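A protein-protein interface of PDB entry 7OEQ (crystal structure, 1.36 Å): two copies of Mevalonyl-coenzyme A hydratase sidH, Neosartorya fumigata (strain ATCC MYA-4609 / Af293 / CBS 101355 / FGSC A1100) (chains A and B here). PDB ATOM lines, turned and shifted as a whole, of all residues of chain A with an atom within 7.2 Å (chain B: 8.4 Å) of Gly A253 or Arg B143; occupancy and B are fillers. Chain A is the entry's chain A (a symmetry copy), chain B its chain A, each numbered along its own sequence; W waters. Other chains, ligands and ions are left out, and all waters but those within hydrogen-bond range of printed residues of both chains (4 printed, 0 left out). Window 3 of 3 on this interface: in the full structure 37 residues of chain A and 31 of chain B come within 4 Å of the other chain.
Asn A208 touches Val B141 (CB to O, 3.3 Å).
Asn A208 touches Gln B142 (OD1 to CG, 3.4 Å).
Ser A209 touches Gly B144 (CB to CA, 3.7 Å).
CA of Val B141 touches CB of Ser A212, at 3.8 Å.
Phe A250 touches Gly B144 (CD1 to O, 3.7 Å).
O of Arg B143 touches CA of Gly A253, 3.6 Å away.
Trp A265 touches Gln B142 (CZ2 to O, 3.4 Å).
Trp A265 touches Arg B143 (CH2 to C, 3.7 Å).
CH2 of Trp A265 touches N of Gly B144, 3.6 Å away.
Water W1 lies within hydrogen-bond range of the backbone carbonyl oxygen of Gly B144 (2.7 Å), the side-chain hydroxyl of Ser A209 (2.8 Å) and the backbone NH of Phe A250 (3.4 Å).
Water W3 lies within hydrogen-bond range of OD1 of Asn A208 (2.7 Å) and OE1 of Gln B142 (3.3 Å).
Water W4 bridges O of Gln B142 and NE1 of Trp A265.
Water W2 bridges the backbone carbonyl oxygen of Ser B170 and the side-chain amide oxygen of Asn A208.
Of the 24 printed residues of chain B, 6 touch a printed residue of chain A.
Among the printed residues, 13 pairs touch across the chains.
Among the printed residues, no Asp or Glu carboxylate lies within 4 Å of a Lys or Arg side-chain nitrogen of the other chain.
O of Val B141 lies within hydrogen-bond range of N of Ser A209 (3.2 Å).
O of Gly B144 sits close to OG of Ser A212, 3.4 Å away.
The backbone carbonyl oxygen (O) of Ile B145 is in hydrogen-bond range of the side-chain hydroxyl (OG) of Ser A212, 2.7 Å away.
The backbone carbonyl oxygen of Ser B170 sits at hydrogen-bond distance from the side-chain amide nitrogen of Asn A208.
Printed residues of chain B within 4 Å of Phe A250: Gly B144 (3.7 Å).
Gly A253 touches one residue of chain B.
Leu B138 touches none of the printed residues of chain A.
Glu B140 touches none of the printed residues of chain A.
Of the printed residues of chain A, Val B141 touches Asn A208, Ser A209 and Ser A212.
Of chain A, only Gly A253 (3.6 Å) and Trp A265 (3.7 Å) come within 4 Å of Arg B143.
Printed residues of chain A within 4 Å of Gly B144: Ser A209, Ser A212, Phe A250 and Trp A265.
Printed residues of chain A within 4 Å of Ile B145: Ser A212.
The nearest residue of chain B that does not touch Gly A253 is Gly B144 (5.1 Å).
The nearest printed residue of chain A that does not touch Ser B170 is Ser A209 (8.3 Å).
No position is printed for both chains.
Of the 13 pairs that touch across the chains among the printed residues, none has its exchanged pair printed and touching as well.
The backbone carbonyl oxygen (O) of Glu B140 lies within hydrogen-bond range of the backbone NH (N) of Ile B145, at 3.2 Å.
The side-chain amide nitrogen of Gln B142 sits at hydrogen-bond distance from the backbone carbonyl oxygen of Gly B171.
The side-chain hydroxyl (OG) of Ser A209 sits at hydrogen-bond distance from the backbone NH (N) of Ser A212 (3.2 Å).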
ATOM      1  N   ASN A 208     -34.736  -2.282  -9.630  1.00  0.00           N
ATOM      2  CA  ASN A 208     -33.430  -2.521 -10.282  1.00  0.00           C
ATOM      3  C   ASN A 208     -32.388  -1.576  -9.684  1.00  0.00           C
ATOM      4  O   ASN A 208     -32.700  -0.594  -9.005  1.00  0.00           O
ATOM      5  CB  ASN A 208     -33.544  -2.444 -11.802  1.00  0.00           C
ATOM      6  CG  ASN A 208     -34.484  -3.529 -12.327  1.00  0.00           C
ATOM      7  OD1 ASN A 208     -34.554  -4.627 -11.762  1.00  0.00           O
ATOM      8  ND2 ASN A 208     -35.202  -3.264 -13.406  1.00  0.00           N
ATOM      9  N   SER A 209     -31.138  -1.830 -10.008  1.00  0.00           N
ATOM     10  CA  SER A 209     -30.065  -0.970  -9.496  1.00  0.00           C
ATOM     11  C   SER A 209     -30.255   0.447 -10.047  1.00  0.00           C
ATOM     12  O   SER A 209     -30.378   0.631 -11.260  1.00  0.00           O
ATOM     13  CB  SER A 209     -28.723  -1.507  -9.854  1.00  0.00           C
ATOM     14  OG  SER A 209     -27.801  -0.442  -9.821  1.00  0.00           O
ATOM     15  N   SER A 212     -27.600   1.099 -12.673  1.00  0.00           N
ATOM     16  CA  SER A 212     -27.946   0.375 -13.912  1.00  0.00           C
ATOM     17  C   SER A 212     -29.016   1.155 -14.699  1.00  0.00           C
ATOM     18  O   SER A 212     -28.947   1.228 -15.927  1.00  0.00           O
ATOM     19  CB  SER A 212     -28.429  -1.027 -13.595  1.00  0.00           C
ATOM     20  OG  SER A 212     -27.462  -1.835 -12.911  1.00  0.00           O
ATOM     21  N   GLU A 248     -20.810   1.263  -5.442  1.00  0.00           N
ATOM     22  CA  GLU A 248     -21.189   0.328  -4.348  1.00  0.00           C
ATOM     23  C   GLU A 248     -22.313  -0.601  -4.845  1.00  0.00           C
ATOM     24  O   GLU A 248     -22.307  -1.799  -4.466  1.00  0.00           O
ATOM     25  CB  GLU A 248     -21.568   1.105  -3.085  1.00  0.00           C
ATOM     26  CG  GLU A 248     -20.383   1.821  -2.456  1.00  0.00           C
ATOM     27  CD  GLU A 248     -19.229   0.894  -2.108  1.00  0.00           C
ATOM     28  OE1 GLU A 248     -19.418   0.034  -1.231  1.00  0.00           O
ATOM     29  OE2 GLU A 248     -18.154   1.004  -2.741  1.00  0.00           O
ATOM     30  N   ASN A 249     -23.221  -0.128  -5.696  1.00  0.00           N
ATOM     31  CA  ASN A 249     -24.358  -0.990  -6.138  1.00  0.00           C
ATOM     32  C   ASN A 249     -23.834  -2.207  -6.921  1.00  0.00           C
ATOM     33  O   ASN A 249     -24.338  -3.322  -6.674  1.00  0.00           O
ATOM     34  CB  ASN A 249     -25.397  -0.232  -6.967  1.00  0.00           C
ATOM     35  CG  ASN A 249     -26.362   0.570  -6.116  1.00  0.00           C
ATOM     36  OD1 ASN A 249     -26.787   0.128  -5.038  1.00  0.00           O
ATOM     37  ND2 ASN A 249     -26.695   1.764  -6.582  1.00  0.00           N
ATOM     38  N   PHE A 250     -22.865  -2.018  -7.835  1.00  0.00           N
ATOM     39  CA  PHE A 250     -22.306  -3.130  -8.650  1.00  0.00           C
ATOM     40  C   PHE A 250     -21.692  -4.176  -7.713  1.00  0.00           C
ATOM     41  O   PHE A 250     -21.906  -5.385  -7.942  1.00  0.00           O
ATOM     42  CB  PHE A 250     -21.287  -2.645  -9.684  1.00  0.00           C
ATOM     43  CG  PHE A 250     -20.524  -3.756 -10.353  1.00  0.00           C
ATOM     44  CD1 PHE A 250     -21.035  -4.423 -11.453  1.00  0.00           C
ATOM     45  CD2 PHE A 250     -19.271  -4.129  -9.892  1.00  0.00           C
ATOM     46  CE1 PHE A 250     -20.327  -5.452 -12.061  1.00  0.00           C
ATOM     47  CE2 PHE A 250     -18.571  -5.163 -10.496  1.00  0.00           C
ATOM     48  CZ  PHE A 250     -19.093  -5.813 -11.587  1.00  0.00           C
ATOM     49  N   HIS A 251     -20.966  -3.742  -6.679  1.00  0.00           N
ATOM     50  CA  HIS A 251     -20.309  -4.667  -5.712  1.00  0.00           C
ATOM     51  C   HIS A 251     -21.392  -5.401  -4.898  1.00  0.00           C
ATOM     52  O   HIS A 251     -21.248  -6.625  -4.670  1.00  0.00           O
ATOM     53  CB  HIS A 251     -19.242  -3.917  -4.901  1.00  0.00           C
ATOM     54  CG  HIS A 251     -18.095  -3.457  -5.747  1.00  0.00           C
ATOM     55  ND1 HIS A 251     -17.134  -4.330  -6.231  1.00  0.00           N
ATOM     56  CD2 HIS A 251     -17.766  -2.235  -6.228  1.00  0.00           C
ATOM     57  CE1 HIS A 251     -16.255  -3.658  -6.951  1.00  0.00           C
ATOM     58  NE2 HIS A 251     -16.622  -2.370  -6.964  1.00  0.00           N
ATOM     59  N   GLU A 252     -22.480  -4.723  -4.530  1.00  0.00           N
ATOM     60  CA  GLU A 252     -23.615  -5.384  -3.838  1.00  0.00           C
ATOM     61  C   GLU A 252     -24.235  -6.434  -4.780  1.00  0.00           C
ATOM     62  O   GLU A 252     -24.577  -7.537  -4.298  1.00  0.00           O
ATOM     63  CB  GLU A 252     -24.641  -4.348  -3.374  1.00  0.00           C
ATOM     64  CG  GLU A 252     -25.972  -4.955  -2.931  1.00  0.00           C
ATOM     65  CD  GLU A 252     -25.921  -5.852  -1.712  1.00  0.00           C
ATOM     66  OE1 GLU A 252     -26.995  -6.345  -1.301  1.00  0.00           O
ATOM     67  OE2 GLU A 252     -24.822  -6.061  -1.170  1.00  0.00           O
ATOM     68  N   GLY A 253     -24.365  -6.120  -6.073  1.00  0.00           N
ATOM     69  CA  GLY A 253     -24.878  -7.083  -7.074  1.00  0.00           C
ATOM     70  C   GLY A 253     -24.059  -8.365  -7.094  1.00  0.00           C
ATOM     71  O   GLY A 253     -24.676  -9.458  -7.197  1.00  0.00           O
ATOM     72  N   VAL A 254     -22.725  -8.238  -6.997  1.00  0.00           N
ATOM     73  CA  VAL A 254     -21.740  -9.359  -7.080  1.00  0.00           C
ATOM     74  C   VAL A 254     -21.731 -10.133  -5.753  1.00  0.00           C
ATOM     75  O   VAL A 254     -21.595 -11.376  -5.805  1.00  0.00           O
ATOM     76  CB  VAL A 254     -20.332  -8.847  -7.449  1.00  0.00           C
ATOM     77  CG1 VAL A 254     -19.263  -9.934  -7.322  1.00  0.00           C
ATOM     78  CG2 VAL A 254     -20.314  -8.240  -8.845  1.00  0.00           C
ATOM     79  N   ARG A 255     -21.858  -9.445  -4.610  1.00  0.00           N
ATOM     80  CA  ARG A 255     -21.930 -10.098  -3.269  1.00  0.00           C
ATOM     81  C   ARG A 255     -23.200 -10.961  -3.212  1.00  0.00           C
ATOM     82  O   ARG A 255     -23.117 -12.091  -2.697  1.00  0.00           O
ATOM     83  CB  ARG A 255     -21.894  -9.059  -2.142  1.00  0.00           C
ATOM     84  N   ALA A 256     -24.312 -10.448  -3.753  1.00  0.00           N
ATOM     85  CA  ALA A 256     -25.656 -11.079  -3.781  1.00  0.00           C
ATOM     86  C   ALA A 256     -25.661 -12.328  -4.679  1.00  0.00           C
ATOM     87  O   ALA A 256     -26.323 -13.331  -4.294  1.00  0.00           O
ATOM     88  CB  ALA A 256     -26.673 -10.059  -4.242  1.00  0.00           C
ATOM     89  N   PHE A 257     -24.971 -12.278  -5.830  1.00  0.00           N
ATOM     90  CA  PHE A 257     -24.761 -13.424  -6.759  1.00  0.00           C
ATOM     91  C   PHE A 257     -23.966 -14.521  -6.047  1.00  0.00           C
ATOM     92  O   PHE A 257     -24.488 -15.650  -5.896  1.00  0.00           O
ATOM     93  CB  PHE A 257     -24.010 -12.993  -8.021  1.00  0.00           C
ATOM     94  N   VAL A 258     -22.744 -14.189  -5.612  1.00  0.00           N
ATOM     95  CA  VAL A 258     -21.818 -15.128  -4.907  1.00  0.00           C
ATOM     96  C   VAL A 258     -22.556 -15.717  -3.700  1.00  0.00           C
ATOM     97  O   VAL A 258     -22.476 -16.940  -3.531  1.00  0.00           O
ATOM     98  CB  VAL A 258     -20.495 -14.452  -4.494  1.00  0.00           C
ATOM     99  N   GLU A 259     -23.282 -14.899  -2.925  1.00  0.00           N
ATOM    100  CA  GLU A 259     -23.971 -15.345  -1.677  1.00  0.00           C
ATOM    101  C   GLU A 259     -25.366 -15.916  -1.980  1.00  0.00           C
ATOM    102  O   GLU A 259     -25.992 -16.433  -1.036  1.00  0.00           O
ATOM    103  CB  GLU A 259     -24.097 -14.196  -0.675  1.00  0.00           C
ATOM    104  CG  GLU A 259     -22.774 -13.740  -0.094  1.00  0.00           C
ATOM    105  CD  GLU A 259     -22.892 -12.506   0.781  1.00  0.00           C
ATOM    106  OE1 GLU A 259     -24.008 -12.239   1.273  1.00  0.00           O
ATOM    107  OE2 GLU A 259     -21.874 -11.809   0.959  1.00  0.00           O
ATOM    108  N   ARG A 261     -28.300 -14.476  -2.660  1.00  0.00           N
ATOM    109  CA  ARG A 261     -29.365 -13.708  -1.947  1.00  0.00           C
ATOM    110  C   ARG A 261     -29.788 -12.505  -2.800  1.00  0.00           C
ATOM    111  O   ARG A 261     -29.138 -12.257  -3.848  1.00  0.00           O
ATOM    112  CB  ARG A 261     -28.874 -13.233  -0.573  1.00  0.00           C
ATOM    113  CG  ARG A 261     -27.714 -12.250  -0.630  1.00  0.00           C
ATOM    114  CD  ARG A 261     -27.441 -11.551   0.687  1.00  0.00           C
ATOM    115  NE  ARG A 261     -26.254 -10.720   0.558  1.00  0.00           N
ATOM    116  CZ  ARG A 261     -26.218  -9.520  -0.019  1.00  0.00           C
ATOM    117  NH1 ARG A 261     -27.319  -8.977  -0.510  1.00  0.00           N
ATOM    118  NH2 ARG A 261     -25.076  -8.862  -0.098  1.00  0.00           N
ATOM    119  N   PRO A 263     -30.227  -8.571  -3.886  1.00  0.00           N
ATOM    120  CA  PRO A 263     -29.411  -7.361  -3.726  1.00  0.00           C
ATOM    121  C   PRO A 263     -30.182  -6.244  -2.998  1.00  0.00           C
ATOM    122  O   PRO A 263     -31.396  -6.154  -3.180  1.00  0.00           O
ATOM    123  CB  PRO A 263     -29.058  -6.982  -5.169  1.00  0.00           C
ATOM    124  CG  PRO A 263     -30.187  -7.537  -6.003  1.00  0.00           C
ATOM    125  CD  PRO A 263     -30.698  -8.770  -5.268  1.00  0.00           C
ATOM    126  N   GLN A 264     -29.485  -5.462  -2.162  1.00  0.00           N
ATOM    127  CA  GLN A 264     -30.036  -4.280  -1.435  1.00  0.00           C
ATOM    128  C   GLN A 264     -29.428  -3.024  -2.057  1.00  0.00           C
ATOM    129  O   GLN A 264     -28.276  -2.705  -1.748  1.00  0.00           O
ATOM    130  CB  GLN A 264     -29.701  -4.307   0.061  1.00  0.00           C
ATOM    131  CG  GLN A 264     -30.288  -5.488   0.813  1.00  0.00           C
ATOM    132  CD  GLN A 264     -31.791  -5.450   0.791  1.00  0.00           C
ATOM    133  OE1 GLN A 264     -32.425  -6.105  -0.028  1.00  0.00           O
ATOM    134  NE2 GLN A 264     -32.364  -4.642   1.667  1.00  0.00           N
ATOM    135  N   TRP A 265     -30.182  -2.329  -2.900  1.00  0.00           N
ATOM    136  CA  TRP A 265     -29.646  -1.191  -3.684  1.00  0.00           C
ATOM    137  C   TRP A 265     -29.638   0.080  -2.827  1.00  0.00           C
ATOM    138  O   TRP A 265     -30.477   0.221  -1.917  1.00  0.00           O
ATOM    139  CB  TRP A 265     -30.435  -0.970  -4.976  1.00  0.00           C
ATOM    140  CG  TRP A 265     -30.581  -2.172  -5.858  1.00  0.00           C
ATOM    141  CD1 TRP A 265     -31.753  -2.700  -6.319  1.00  0.00           C
ATOM    142  CD2 TRP A 265     -29.532  -2.961  -6.438  1.00  0.00           C
ATOM    143  NE1 TRP A 265     -31.500  -3.786  -7.118  1.00  0.00           N
ATOM    144  CE2 TRP A 265     -30.144  -3.961  -7.221  1.00  0.00           C
ATOM    145  CE3 TRP A 265     -28.141  -2.934  -6.372  1.00  0.00           C
ATOM    146  CZ2 TRP A 265     -29.411  -4.916  -7.933  1.00  0.00           C
ATOM    147  CZ3 TRP A 265     -27.419  -3.881  -7.069  1.00  0.00           C
ATOM    148  CH2 TRP A 265     -28.048  -4.860  -7.833  1.00  0.00           C
ATOM    149  N   CYS B  34     -24.936 -20.516 -22.281  1.00  0.00           N
ATOM    150  CA  CYS B  34     -24.021 -19.384 -21.988  1.00  0.00           C
ATOM    151  C   CYS B  34     -22.700 -19.637 -22.704  1.00  0.00           C
ATOM    152  O   CYS B  34     -22.329 -20.792 -22.895  1.00  0.00           O
ATOM    153  CB  CYS B  34     -23.830 -19.185 -20.496  1.00  0.00           C
ATOM    154  SG  CYS B  34     -25.339 -18.615 -19.671  1.00  0.00           S
ATOM    155  N   ALA B  70     -28.202 -17.688 -23.027  1.00  0.00           N
ATOM    156  CA  ALA B  70     -28.443 -16.848 -21.840  1.00  0.00           C
ATOM    157  C   ALA B  70     -27.287 -15.859 -21.593  1.00  0.00           C
ATOM    158  O   ALA B  70     -27.284 -15.235 -20.545  1.00  0.00           O
ATOM    159  CB  ALA B  70     -28.803 -17.723 -20.655  1.00  0.00           C
ATOM    160  N   GLY B  71     -26.383 -15.671 -22.564  1.00  0.00           N
ATOM    161  CA  GLY B  71     -25.335 -14.635 -22.537  1.00  0.00           C
ATOM    162  C   GLY B  71     -23.996 -15.186 -22.113  1.00  0.00           C
ATOM    163  O   GLY B  71     -23.661 -16.354 -22.405  1.00  0.00           O
ATOM    164  N   ALA B  72     -23.189 -14.313 -21.533  1.00  0.00           N
ATOM    165  CA  ALA B  72     -21.827 -14.663 -21.116  1.00  0.00           C
ATOM    166  C   ALA B  72     -21.865 -15.674 -19.961  1.00  0.00           C
ATOM    167  O   ALA B  72     -22.794 -15.646 -19.151  1.00  0.00           O
ATOM    168  CB  ALA B  72     -21.112 -13.391 -20.741  1.00  0.00           C
ATOM    169  N   ASP B  73     -20.840 -16.512 -19.857  1.00  0.00           N
ATOM    170  CA  ASP B  73     -20.657 -17.386 -18.675  1.00  0.00           C
ATOM    171  C   ASP B  73     -20.431 -16.489 -17.448  1.00  0.00           C
ATOM    172  O   ASP B  73     -19.349 -15.881 -17.348  1.00  0.00           O
ATOM    173  CB  ASP B  73     -19.562 -18.402 -18.972  1.00  0.00           C
ATOM    174  CG  ASP B  73     -19.272 -19.345 -17.837  1.00  0.00           C
ATOM    175  OD1 ASP B  73     -19.488 -18.950 -16.675  1.00  0.00           O
ATOM    176  OD2 ASP B  73     -18.828 -20.456 -18.135  1.00  0.00           O
ATOM    177  N   LEU B  74     -21.410 -16.437 -16.527  1.00  0.00           N
ATOM    178  CA  LEU B  74     -21.398 -15.479 -15.383  1.00  0.00           C
ATOM    179  C   LEU B  74     -20.436 -15.962 -14.282  1.00  0.00           C
ATOM    180  O   LEU B  74     -19.901 -15.094 -13.540  1.00  0.00           O
ATOM    181  CB  LEU B  74     -22.820 -15.259 -14.845  1.00  0.00           C
ATOM    182  CG  LEU B  74     -23.741 -14.388 -15.704  1.00  0.00           C
ATOM    183  CD1 LEU B  74     -25.043 -14.093 -14.971  1.00  0.00           C
ATOM    184  CD2 LEU B  74     -23.071 -13.083 -16.123  1.00  0.00           C
ATOM    185  N   TRP B  77     -17.145 -14.577 -15.673  1.00  0.00           N
ATOM    186  CA  TRP B  77     -17.159 -13.087 -15.579  1.00  0.00           C
ATOM    187  C   TRP B  77     -16.990 -12.670 -14.111  1.00  0.00           C
ATOM    188  O   TRP B  77     -16.278 -11.684 -13.874  1.00  0.00           O
ATOM    189  CB  TRP B  77     -18.425 -12.482 -16.207  1.00  0.00           C
ATOM    190  N   LEU B 115     -31.356 -14.224 -23.618  1.00  0.00           N
ATOM    191  CA  LEU B 115     -31.222 -13.338 -22.437  1.00  0.00           C
ATOM    192  C   LEU B 115     -29.826 -12.675 -22.400  1.00  0.00           C
ATOM    193  O   LEU B 115     -28.807 -13.352 -22.660  1.00  0.00           O
ATOM    194  CB  LEU B 115     -31.445 -14.123 -21.143  1.00  0.00           C
ATOM    195  CG  LEU B 115     -32.776 -14.862 -20.997  1.00  0.00           C
ATOM    196  CD1 LEU B 115     -32.761 -15.697 -19.726  1.00  0.00           C
ATOM    197  CD2 LEU B 115     -33.927 -13.875 -20.988  1.00  0.00           C
ATOM    198  N   GLY B 116     -29.812 -11.411 -22.002  1.00  0.00           N
ATOM    199  CA  GLY B 116     -28.551 -10.703 -21.748  1.00  0.00           C
ATOM    200  C   GLY B 116     -27.727 -10.649 -23.026  1.00  0.00           C
ATOM    201  O   GLY B 116     -28.236 -10.226 -24.064  1.00  0.00           O
ATOM    202  N   GLY B 117     -26.465 -11.073 -22.945  1.00  0.00           N
ATOM    203  CA  GLY B 117     -25.601 -11.070 -24.140  1.00  0.00           C
ATOM    204  C   GLY B 117     -26.229 -11.843 -25.295  1.00  0.00           C
ATOM    205  O   GLY B 117     -25.998 -11.528 -26.470  1.00  0.00           O
ATOM    206  N   GLY B 118     -27.039 -12.892 -24.988  1.00  0.00           N
ATOM    207  CA  GLY B 118     -27.696 -13.612 -26.087  1.00  0.00           C
ATOM    208  C   GLY B 118     -28.701 -12.773 -26.863  1.00  0.00           C
ATOM    209  O   GLY B 118     -28.802 -12.897 -28.078  1.00  0.00           O
ATOM    210  N   GLY B 137     -34.950 -11.043 -23.157  1.00  0.00           N
ATOM    211  CA  GLY B 137     -34.829 -10.099 -22.041  1.00  0.00           C
ATOM    212  C   GLY B 137     -33.398  -9.627 -21.864  1.00  0.00           C
ATOM    213  O   GLY B 137     -32.511 -10.349 -22.321  1.00  0.00           O
ATOM    214  N   LEU B 138     -33.277  -8.516 -21.154  1.00  0.00           N
ATOM    215  CA  LEU B 138     -31.977  -7.934 -20.713  1.00  0.00           C
ATOM    216  C   LEU B 138     -31.983  -7.815 -19.198  1.00  0.00           C
ATOM    217  O   LEU B 138     -32.254  -6.751 -18.657  1.00  0.00           O
ATOM    218  CB  LEU B 138     -31.771  -6.581 -21.381  1.00  0.00           C
ATOM    219  CG  LEU B 138     -31.630  -6.565 -22.900  1.00  0.00           C
ATOM    220  CD1 LEU B 138     -31.596  -5.110 -23.382  1.00  0.00           C
ATOM    221  CD2 LEU B 138     -30.409  -7.363 -23.358  1.00  0.00           C
ATOM    222  N   PRO B 139     -31.758  -8.917 -18.448  1.00  0.00           N
ATOM    223  CA  PRO B 139     -31.828  -8.861 -16.979  1.00  0.00           C
ATOM    224  C   PRO B 139     -30.639  -8.152 -16.305  1.00  0.00           C
ATOM    225  O   PRO B 139     -30.628  -8.084 -15.096  1.00  0.00           O
ATOM    226  CB  PRO B 139     -31.944 -10.344 -16.592  1.00  0.00           C
ATOM    227  CG  PRO B 139     -31.272 -11.101 -17.717  1.00  0.00           C
ATOM    228  CD  PRO B 139     -31.460 -10.266 -18.959  1.00  0.00           C
ATOM    229  N   GLU B 140     -29.706  -7.600 -17.087  1.00  0.00           N
ATOM    230  CA  GLU B 140     -28.515  -6.866 -16.572  1.00  0.00           C
ATOM    231  C   GLU B 140     -28.940  -5.893 -15.468  1.00  0.00           C
ATOM    232  O   GLU B 140     -28.286  -5.875 -14.396  1.00  0.00           O
ATOM    233  CB  GLU B 140     -27.830  -6.151 -17.731  1.00  0.00           C
ATOM    234  CG  GLU B 140     -26.941  -7.033 -18.585  1.00  0.00           C
ATOM    235  CD  GLU B 140     -27.624  -7.843 -19.674  1.00  0.00           C
ATOM    236  OE1 GLU B 140     -28.900  -7.834 -19.733  1.00  0.00           O
ATOM    237  OE2 GLU B 140     -26.873  -8.486 -20.457  1.00  0.00           O
ATOM    238  N   VAL B 141     -29.986  -5.096 -15.698  1.00  0.00           N
ATOM    239  CA  VAL B 141     -30.395  -4.036 -14.725  1.00  0.00           C
ATOM    240  C   VAL B 141     -30.798  -4.674 -13.382  1.00  0.00           C
ATOM    241  O   VAL B 141     -30.643  -3.995 -12.357  1.00  0.00           O
ATOM    242  CB  VAL B 141     -31.533  -3.145 -15.243  1.00  0.00           C
ATOM    243  CG1 VAL B 141     -31.078  -2.155 -16.278  1.00  0.00           C
ATOM    244  CG2 VAL B 141     -32.754  -3.960 -15.704  1.00  0.00           C
ATOM    245  N   GLN B 142     -31.256  -5.931 -13.359  1.00  0.00           N
ATOM    246  CA  GLN B 142     -31.676  -6.604 -12.101  1.00  0.00           C
ATOM    247  C   GLN B 142     -30.454  -7.049 -11.277  1.00  0.00           C
ATOM    248  O   GLN B 142     -30.638  -7.316 -10.069  1.00  0.00           O
ATOM    249  CB  GLN B 142     -32.529  -7.845 -12.356  1.00  0.00           C
ATOM    250  CG  GLN B 142     -33.735  -7.621 -13.267  1.00  0.00           C
ATOM    251  CD  GLN B 142     -34.755  -8.712 -13.078  1.00  0.00           C
ATOM    252  OE1 GLN B 142     -35.116  -9.048 -11.959  1.00  0.00           O
ATOM    253  NE2 GLN B 142     -35.207  -9.286 -14.178  1.00  0.00           N
ATOM    254  N   ARG B 143     -29.281  -7.156 -11.910  1.00  0.00           N
ATOM    255  CA  ARG B 143     -28.035  -7.680 -11.284  1.00  0.00           C
ATOM    256  C   ARG B 143     -27.016  -6.546 -11.016  1.00  0.00           C
ATOM    257  O   ARG B 143     -25.927  -6.842 -10.523  1.00  0.00           O
ATOM    258  CB  ARG B 143     -27.381  -8.741 -12.190  1.00  0.00           C
ATOM    259  CG  ARG B 143     -28.334  -9.740 -12.846  1.00  0.00           C
ATOM    260  CD  ARG B 143     -27.553 -10.814 -13.609  1.00  0.00           C
ATOM    261  NE  ARG B 143     -27.916 -11.021 -15.021  1.00  0.00           N
ATOM    262  CZ  ARG B 143     -27.097 -10.854 -16.079  1.00  0.00           C
ATOM    263  NH1 ARG B 143     -27.540 -11.087 -17.312  1.00  0.00           N
ATOM    264  NH2 ARG B 143     -25.841 -10.457 -15.907  1.00  0.00           N
ATOM    265  N   GLY B 144     -27.326  -5.291 -11.332  1.00  0.00           N
ATOM    266  CA  GLY B 144     -26.404  -4.174 -11.037  1.00  0.00           C
ATOM    267  C   GLY B 144     -25.428  -3.875 -12.156  1.00  0.00           C
ATOM    268  O   GLY B 144     -24.477  -3.121 -11.907  1.00  0.00           O
ATOM    269  N   ILE B 145     -25.633  -4.416 -13.348  1.00  0.00           N
ATOM    270  CA  ILE B 145     -24.803  -4.047 -14.534  1.00  0.00           C
ATOM    271  C   ILE B 145     -25.759  -3.473 -15.596  1.00  0.00           C
ATOM    272  O   ILE B 145     -26.832  -2.995 -15.221  1.00  0.00           O
ATOM    273  CB  ILE B 145     -23.900  -5.221 -14.989  1.00  0.00           C
ATOM    274  CG1 ILE B 145     -22.583  -4.749 -15.620  1.00  0.00           C
ATOM    275  CG2 ILE B 145     -24.631  -6.210 -15.883  1.00  0.00           C
ATOM    276  CD1 ILE B 145     -21.652  -5.880 -16.024  1.00  0.00           C
ATOM    277  N   ALA B 146     -25.364  -3.417 -16.853  1.00  0.00           N
ATOM    278  CA  ALA B 146     -26.202  -2.828 -17.909  1.00  0.00           C
ATOM    279  C   ALA B 146     -25.847  -3.515 -19.215  1.00  0.00           C
ATOM    280  O   ALA B 146     -24.745  -4.127 -19.287  1.00  0.00           O
ATOM    281  CB  ALA B 146     -26.007  -1.336 -17.969  1.00  0.00           C
ATOM    282  N   ALA B 147     -26.759  -3.444 -20.180  1.00  0.00           N
ATOM    283  CA  ALA B 147     -26.562  -4.034 -21.511  1.00  0.00           C
ATOM    284  C   ALA B 147     -25.683  -3.069 -22.300  1.00  0.00           C
ATOM    285  O   ALA B 147     -26.235  -2.132 -22.888  1.00  0.00           O
ATOM    286  CB  ALA B 147     -27.911  -4.296 -22.149  1.00  0.00           C
ATOM    287  N   SER B 170     -36.829  -2.433 -17.430  1.00  0.00           N
ATOM    288  CA  SER B 170     -37.522  -3.394 -16.543  1.00  0.00           C
ATOM    289  C   SER B 170     -36.661  -4.632 -16.257  1.00  0.00           C
ATOM    290  O   SER B 170     -36.737  -5.153 -15.141  1.00  0.00           O
ATOM    291  CB  SER B 170     -38.870  -3.820 -17.081  1.00  0.00           C
ATOM    292  OG  SER B 170     -38.750  -4.718 -18.188  1.00  0.00           O
ATOM    293  N   GLY B 171     -35.887  -5.095 -17.230  1.00  0.00           N
ATOM    294  CA  GLY B 171     -35.153  -6.359 -17.147  1.00  0.00           C
ATOM    295  C   GLY B 171     -36.022  -7.588 -17.186  1.00  0.00           C
ATOM    296  O   GLY B 171     -35.447  -8.673 -16.912  1.00  0.00           O
HETATM  297  O   HOH W   1     -25.141  -1.174 -10.162  1.00  0.00           O
HETATM  298  O   HOH W   2     -37.690  -5.727 -12.443  1.00  0.00           O
HETATM  299  O   HOH W   3     -34.966  -6.506  -9.857  1.00  0.00           O
HETATM  300  O   HOH W   4     -32.764  -6.301  -8.522  1.00  0.00           O
